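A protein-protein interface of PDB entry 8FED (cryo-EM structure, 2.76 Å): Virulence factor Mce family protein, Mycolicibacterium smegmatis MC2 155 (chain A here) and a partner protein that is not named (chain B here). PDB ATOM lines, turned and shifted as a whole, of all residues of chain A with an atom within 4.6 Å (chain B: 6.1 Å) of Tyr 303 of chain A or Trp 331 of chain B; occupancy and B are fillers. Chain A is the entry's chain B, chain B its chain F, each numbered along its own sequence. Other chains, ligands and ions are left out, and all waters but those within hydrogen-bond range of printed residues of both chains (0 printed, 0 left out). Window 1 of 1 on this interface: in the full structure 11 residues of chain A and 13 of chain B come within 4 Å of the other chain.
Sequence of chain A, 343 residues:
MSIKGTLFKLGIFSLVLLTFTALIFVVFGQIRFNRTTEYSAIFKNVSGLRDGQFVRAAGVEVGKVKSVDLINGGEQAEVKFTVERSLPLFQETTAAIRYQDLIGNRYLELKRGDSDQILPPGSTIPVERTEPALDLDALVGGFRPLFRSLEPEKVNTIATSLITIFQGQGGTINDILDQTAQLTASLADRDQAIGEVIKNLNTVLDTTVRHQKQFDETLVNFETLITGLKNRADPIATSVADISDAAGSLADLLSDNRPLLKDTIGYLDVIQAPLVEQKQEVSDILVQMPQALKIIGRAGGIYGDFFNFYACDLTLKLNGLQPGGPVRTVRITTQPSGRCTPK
The backbone NH (N) of Leu 326 of chain B lies within hydrogen-bond range of the backbone carbonyl oxygen (O) of Ile 302 of chain A, at 3.0 Å. The side-chain hydroxyl of Tyr 303 of chain A lies within hydrogen-bond range of the backbone NH of Arg 332 of chain B, 3.0 Å away.
The backbone NH (N) of Gly 301 of chain A lies within hydrogen-bond range of the backbone carbonyl oxygen (O) of Phe 306 of chain A (3.2 Å).
Among the printed residues, pairs that only touch across the chains: Gly 304 of chain A with Phe 325 of chain B (3.2 Å), Gly 301 of chain A with Phe 325 of chain B (3.2 Å), Tyr 303 of chain A with Trp 331 of chain B (3.3 Å), Ile 302 of chain A with Phe 325 of chain B (3.5 Å), Tyr 303 of chain A with Leu 326 of chain B (3.6 Å), Tyr 303 of chain A with Leu 322 of chain B (3.7 Å), Gly 304 of chain A with Leu 322 of chain B (3.7 Å), Phe 306 of chain A with Leu 322 of chain B (3.7 Å), Phe 306 of chain A with Trp 331 of chain B (3.8 Å) and Gly 304 of chain A with Cys 321 of chain B (3.9 Å).
Tyr 303 of chain A touches four residues of chain B. Trp 331 of chain B touches just these residues of chain A: Tyr 303 and Phe 306. Printed residues of chain B within 4 Å of Gly 301 of chain A: Phe 325. Of the printed residues of chain B, Ile 302 of chain A touches Phe 325 (3.5 Å) and Leu 326 (3.0 Å). Printed residues of chain B within 4 Å of Phe 306 of chain A: Leu 322 and Trp 331. Printed residues of chain A within 4 Å of Arg 332 of chain B: Tyr 303. Ala 328 of chain B touches none of the printed residues of chain A. Asn 308 of chain A touches none of the printed residues of chain B. The nearest residue of chain B that does not touch Tyr 303 of chain A is Phe 325 of chain B (4.1 Å). The nearest printed residue of chain A that does not touch Trp 331 of chain B is Gly 304 of chain A (5.3 Å).
Of the 11 printed residues of chain B, 6 touch a printed residue of chain A. Printed residues of chain B that touch a printed residue of chain A: Cys 321, Leu 322, Phe 325, Leu 326, Trp 331 and Arg 332. Hydrophobic or aromatic side chains of chain B that line the printed part of chain A: Leu 322, Phe 325, Leu 326 and Trp 331. Among the printed residues, no Asp or Glu carboxylate lies within 4 Å of a Lys or Arg side-chain nitrogen of the other chain.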
ATOM      1  N   GLY A 301      24.621 -10.028 -17.478  1.00  0.00           N
ATOM      2  CA  GLY A 301      25.472 -11.095 -16.998  1.00  0.00           C
ATOM      3  C   GLY A 301      25.426 -11.340 -15.506  1.00  0.00           C
ATOM      4  O   GLY A 301      26.195 -12.175 -15.011  1.00  0.00           O
ATOM      5  N   ILE A 302      24.560 -10.646 -14.773  1.00  0.00           N
ATOM      6  CA  ILE A 302      24.430 -10.857 -13.336  1.00  0.00           C
ATOM      7  C   ILE A 302      23.196 -11.692 -13.021  1.00  0.00           C
ATOM      8  O   ILE A 302      23.183 -12.447 -12.043  1.00  0.00           O
ATOM      9  CB  ILE A 302      24.397  -9.516 -12.579  1.00  0.00           C
ATOM     10  CG1 ILE A 302      23.210  -8.664 -13.027  1.00  0.00           C
ATOM     11  CG2 ILE A 302      25.699  -8.763 -12.783  1.00  0.00           C
ATOM     12  CD1 ILE A 302      22.972  -7.458 -12.160  1.00  0.00           C
ATOM     13  N   TYR A 303      22.149 -11.568 -13.836  1.00  0.00           N
ATOM     14  CA  TYR A 303      20.935 -12.338 -13.605  1.00  0.00           C
ATOM     15  C   TYR A 303      21.005 -13.748 -14.171  1.00  0.00           C
ATOM     16  O   TYR A 303      20.099 -14.545 -13.910  1.00  0.00           O
ATOM     17  CB  TYR A 303      19.725 -11.615 -14.200  1.00  0.00           C
ATOM     18  CG  TYR A 303      19.355 -10.326 -13.500  1.00  0.00           C
ATOM     19  CD1 TYR A 303      19.866 -10.016 -12.249  1.00  0.00           C
ATOM     20  CD2 TYR A 303      18.480  -9.426 -14.089  1.00  0.00           C
ATOM     21  CE1 TYR A 303      19.522  -8.841 -11.611  1.00  0.00           C
ATOM     22  CE2 TYR A 303      18.130  -8.253 -13.460  1.00  0.00           C
ATOM     23  CZ  TYR A 303      18.654  -7.964 -12.222  1.00  0.00           C
ATOM     24  OH  TYR A 303      18.305  -6.792 -11.593  1.00  0.00           O
ATOM     25  N   GLY A 304      22.040 -14.075 -14.928  1.00  0.00           N
ATOM     26  CA  GLY A 304      22.136 -15.398 -15.518  1.00  0.00           C
ATOM     27  C   GLY A 304      23.133 -15.407 -16.664  1.00  0.00           C
ATOM     28  O   GLY A 304      24.138 -14.699 -16.634  1.00  0.00           O
ATOM     29  N   PHE A 306      22.635 -14.296 -19.672  1.00  0.00           N
ATOM     30  CA  PHE A 306      22.070 -13.429 -20.696  1.00  0.00           C
ATOM     31  C   PHE A 306      22.327 -11.965 -20.373  1.00  0.00           C
ATOM     32  O   PHE A 306      22.494 -11.588 -19.211  1.00  0.00           O
ATOM     33  CB  PHE A 306      20.564 -13.679 -20.846  1.00  0.00           C
ATOM     34  CG  PHE A 306      19.822 -13.723 -19.539  1.00  0.00           C
ATOM     35  CD1 PHE A 306      19.434 -12.558 -18.900  1.00  0.00           C
ATOM     36  CD2 PHE A 306      19.500 -14.935 -18.957  1.00  0.00           C
ATOM     37  CE1 PHE A 306      18.751 -12.600 -17.703  1.00  0.00           C
ATOM     38  CE2 PHE A 306      18.815 -14.983 -17.760  1.00  0.00           C
ATOM     39  CZ  PHE A 306      18.440 -13.813 -17.132  1.00  0.00           C
ATOM     40  N   ASN A 308      20.876  -8.040 -20.326  1.00  0.00           N
ATOM     41  CA  ASN A 308      19.601  -7.418 -19.991  1.00  0.00           C
ATOM     42  C   ASN A 308      19.318  -6.282 -20.965  1.00  0.00           C
ATOM     43  O   ASN A 308      20.046  -5.285 -20.986  1.00  0.00           O
ATOM     44  CB  ASN A 308      19.604  -6.898 -18.556  1.00  0.00           C
ATOM     45  CG  ASN A 308      19.491  -8.004 -17.537  1.00  0.00           C
ATOM     46  OD1 ASN A 308      20.482  -8.638 -17.176  1.00  0.00           O
ATOM     47  ND2 ASN A 308      18.278  -8.244 -17.063  1.00  0.00           N
ATOM     48  N   CYS B 321      22.027 -20.733 -18.210  1.00  0.00           N
ATOM     49  CA  CYS B 321      22.415 -21.311 -16.928  1.00  0.00           C
ATOM     50  C   CYS B 321      22.299 -20.234 -15.858  1.00  0.00           C
ATOM     51  O   CYS B 321      23.053 -19.257 -15.864  1.00  0.00           O
ATOM     52  CB  CYS B 321      23.823 -21.902 -16.962  1.00  0.00           C
ATOM     53  SG  CYS B 321      25.069 -21.044 -17.939  1.00  0.00           S
ATOM     54  N   LEU B 322      21.351 -20.414 -14.945  1.00  0.00           N
ATOM     55  CA  LEU B 322      21.199 -19.551 -13.784  1.00  0.00           C
ATOM     56  C   LEU B 322      21.952 -20.082 -12.572  1.00  0.00           C
ATOM     57  O   LEU B 322      21.787 -19.551 -11.470  1.00  0.00           O
ATOM     58  CB  LEU B 322      19.718 -19.380 -13.447  1.00  0.00           C
ATOM     59  CG  LEU B 322      18.806 -19.032 -14.624  1.00  0.00           C
ATOM     60  CD1 LEU B 322      17.383 -18.803 -14.151  1.00  0.00           C
ATOM     61  CD2 LEU B 322      19.326 -17.814 -15.358  1.00  0.00           C
ATOM     62  N   PHE B 325      24.745 -17.502 -10.580  1.00  0.00           N
ATOM     63  CA  PHE B 325      24.431 -16.097 -10.780  1.00  0.00           C
ATOM     64  C   PHE B 325      23.505 -15.630  -9.659  1.00  0.00           C
ATOM     65  O   PHE B 325      23.274 -16.345  -8.680  1.00  0.00           O
ATOM     66  CB  PHE B 325      23.818 -15.875 -12.164  1.00  0.00           C
ATOM     67  CG  PHE B 325      24.775 -16.123 -13.294  1.00  0.00           C
ATOM     68  CD1 PHE B 325      25.677 -15.149 -13.682  1.00  0.00           C
ATOM     69  CD2 PHE B 325      24.772 -17.329 -13.970  1.00  0.00           C
ATOM     70  CE1 PHE B 325      26.558 -15.377 -14.719  1.00  0.00           C
ATOM     71  CE2 PHE B 325      25.651 -17.559 -15.009  1.00  0.00           C
ATOM     72  CZ  PHE B 325      26.542 -16.582 -15.384  1.00  0.00           C
ATOM     73  N   LEU B 326      22.994 -14.413  -9.799  1.00  0.00           N
ATOM     74  CA  LEU B 326      22.192 -13.809  -8.747  1.00  0.00           C
ATOM     75  C   LEU B 326      20.922 -14.626  -8.516  1.00  0.00           C
ATOM     76  O   LEU B 326      20.369 -15.191  -9.466  1.00  0.00           O
ATOM     77  CB  LEU B 326      21.831 -12.369  -9.120  1.00  0.00           C
ATOM     78  CG  LEU B 326      21.576 -11.370  -7.992  1.00  0.00           C
ATOM     79  CD1 LEU B 326      22.842 -11.155  -7.180  1.00  0.00           C
ATOM     80  CD2 LEU B 326      21.055 -10.052  -8.543  1.00  0.00           C
ATOM     81  N   PRO B 327      20.458 -14.740  -7.271  1.00  0.00           N
ATOM     82  CA  PRO B 327      19.206 -15.460  -7.013  1.00  0.00           C
ATOM     83  C   PRO B 327      18.028 -14.810  -7.720  1.00  0.00           C
ATOM     84  O   PRO B 327      17.982 -13.593  -7.911  1.00  0.00           O
ATOM     85  CB  PRO B 327      19.057 -15.376  -5.490  1.00  0.00           C
ATOM     86  CG  PRO B 327      20.447 -15.217  -4.992  1.00  0.00           C
ATOM     87  CD  PRO B 327      21.152 -14.383  -6.023  1.00  0.00           C
ATOM     88  N   ALA B 328      17.067 -15.650  -8.115  1.00  0.00           N
ATOM     89  CA  ALA B 328      15.917 -15.183  -8.880  1.00  0.00           C
ATOM     90  C   ALA B 328      15.066 -14.185  -8.107  1.00  0.00           C
ATOM     91  O   ALA B 328      14.352 -13.390  -8.725  1.00  0.00           O
ATOM     92  CB  ALA B 328      15.061 -16.374  -9.315  1.00  0.00           C
ATOM     93  N   SER B 329      15.118 -14.211  -6.776  1.00  0.00           N
ATOM     94  CA  SER B 329      14.393 -13.244  -5.966  1.00  0.00           C
ATOM     95  C   SER B 329      15.167 -11.951  -5.752  1.00  0.00           C
ATOM     96  O   SER B 329      14.598 -10.986  -5.231  1.00  0.00           O
ATOM     97  CB  SER B 329      14.035 -13.848  -4.605  1.00  0.00           C
ATOM     98  OG  SER B 329      13.410 -12.886  -3.773  1.00  0.00           O
ATOM     99  N   GLN B 330      16.441 -11.909  -6.136  1.00  0.00           N
ATOM    100  CA  GLN B 330      17.263 -10.714  -6.000  1.00  0.00           C
ATOM    101  C   GLN B 330      17.235  -9.829  -7.239  1.00  0.00           C
ATOM    102  O   GLN B 330      17.924  -8.805  -7.264  1.00  0.00           O
ATOM    103  CB  GLN B 330      18.711 -11.100  -5.681  1.00  0.00           C
ATOM    104  CG  GLN B 330      18.888 -11.852  -4.369  1.00  0.00           C
ATOM    105  CD  GLN B 330      18.546 -11.012  -3.155  1.00  0.00           C
ATOM    106  OE1 GLN B 330      18.660  -9.786  -3.178  1.00  0.00           O
ATOM    107  NE2 GLN B 330      18.122 -11.670  -2.083  1.00  0.00           N
ATOM    108  N   TRP B 331      16.472 -10.202  -8.265  1.00  0.00           N
ATOM    109  CA  TRP B 331      16.344  -9.366  -9.450  1.00  0.00           C
ATOM    110  C   TRP B 331      15.604  -8.079  -9.106  1.00  0.00           C
ATOM    111  O   TRP B 331      14.599  -8.094  -8.390  1.00  0.00           O
ATOM    112  CB  TRP B 331      15.608 -10.118 -10.562  1.00  0.00           C
ATOM    113  CG  TRP B 331      16.354 -11.307 -11.112  1.00  0.00           C
ATOM    114  CD1 TRP B 331      17.510 -11.851 -10.631  1.00  0.00           C
ATOM    115  CD2 TRP B 331      15.988 -12.093 -12.253  1.00  0.00           C
ATOM    116  NE1 TRP B 331      17.885 -12.925 -11.400  1.00  0.00           N
ATOM    117  CE2 TRP B 331      16.968 -13.095 -12.402  1.00  0.00           C
ATOM    118  CE3 TRP B 331      14.929 -12.047 -13.163  1.00  0.00           C
ATOM    119  CZ2 TRP B 331      16.919 -14.041 -13.423  1.00  0.00           C
ATOM    120  CZ3 TRP B 331      14.882 -12.988 -14.176  1.00  0.00           C
ATOM    121  CH2 TRP B 331      15.871 -13.972 -14.298  1.00  0.00           C
ATOM    122  N   ARG B 332      16.107  -6.960  -9.618  1.00  0.00           N
ATOM    123  CA  ARG B 332      15.584  -5.648  -9.277  1.00  0.00           C
ATOM    124  C   ARG B 332      14.580  -5.173 -10.319  1.00  0.00           C
ATOM    125  O   ARG B 332      14.682  -5.496 -11.505  1.00  0.00           O
ATOM    126  CB  ARG B 332      16.716  -4.625  -9.150  1.00  0.00           C
ATOM    127  CG  ARG B 332      17.878  -5.086  -8.287  1.00  0.00           C
ATOM    128  CD  ARG B 332      18.717  -3.924  -7.769  1.00  0.00           C
ATOM    129  NE  ARG B 332      19.158  -3.021  -8.826  1.00  0.00           N
ATOM    130  CZ  ARG B 332      18.654  -1.812  -9.040  1.00  0.00           C
ATOM    131  NH1 ARG B 332      17.684  -1.325  -8.285  1.00  0.00           N
ATOM    132  NH2 ARG B 332      19.138  -1.074 -10.034  1.00  0.00           N
ATOM    133  N   SER B 333      13.602  -4.400  -9.855  1.00  0.00           N
ATOM    134  CA  SER B 333      12.579  -3.870 -10.738  1.00  0.00           C
ATOM    135  C   SER B 333      13.185  -2.837 -11.688  1.00  0.00           C
ATOM    136  O   SER B 333      14.108  -2.109 -11.317  1.00  0.00           O
ATOM    137  CB  SER B 333      11.456  -3.234  -9.922  1.00  0.00           C
ATOM    138  OG  SER B 333      10.479  -2.642 -10.760  1.00  0.00           O
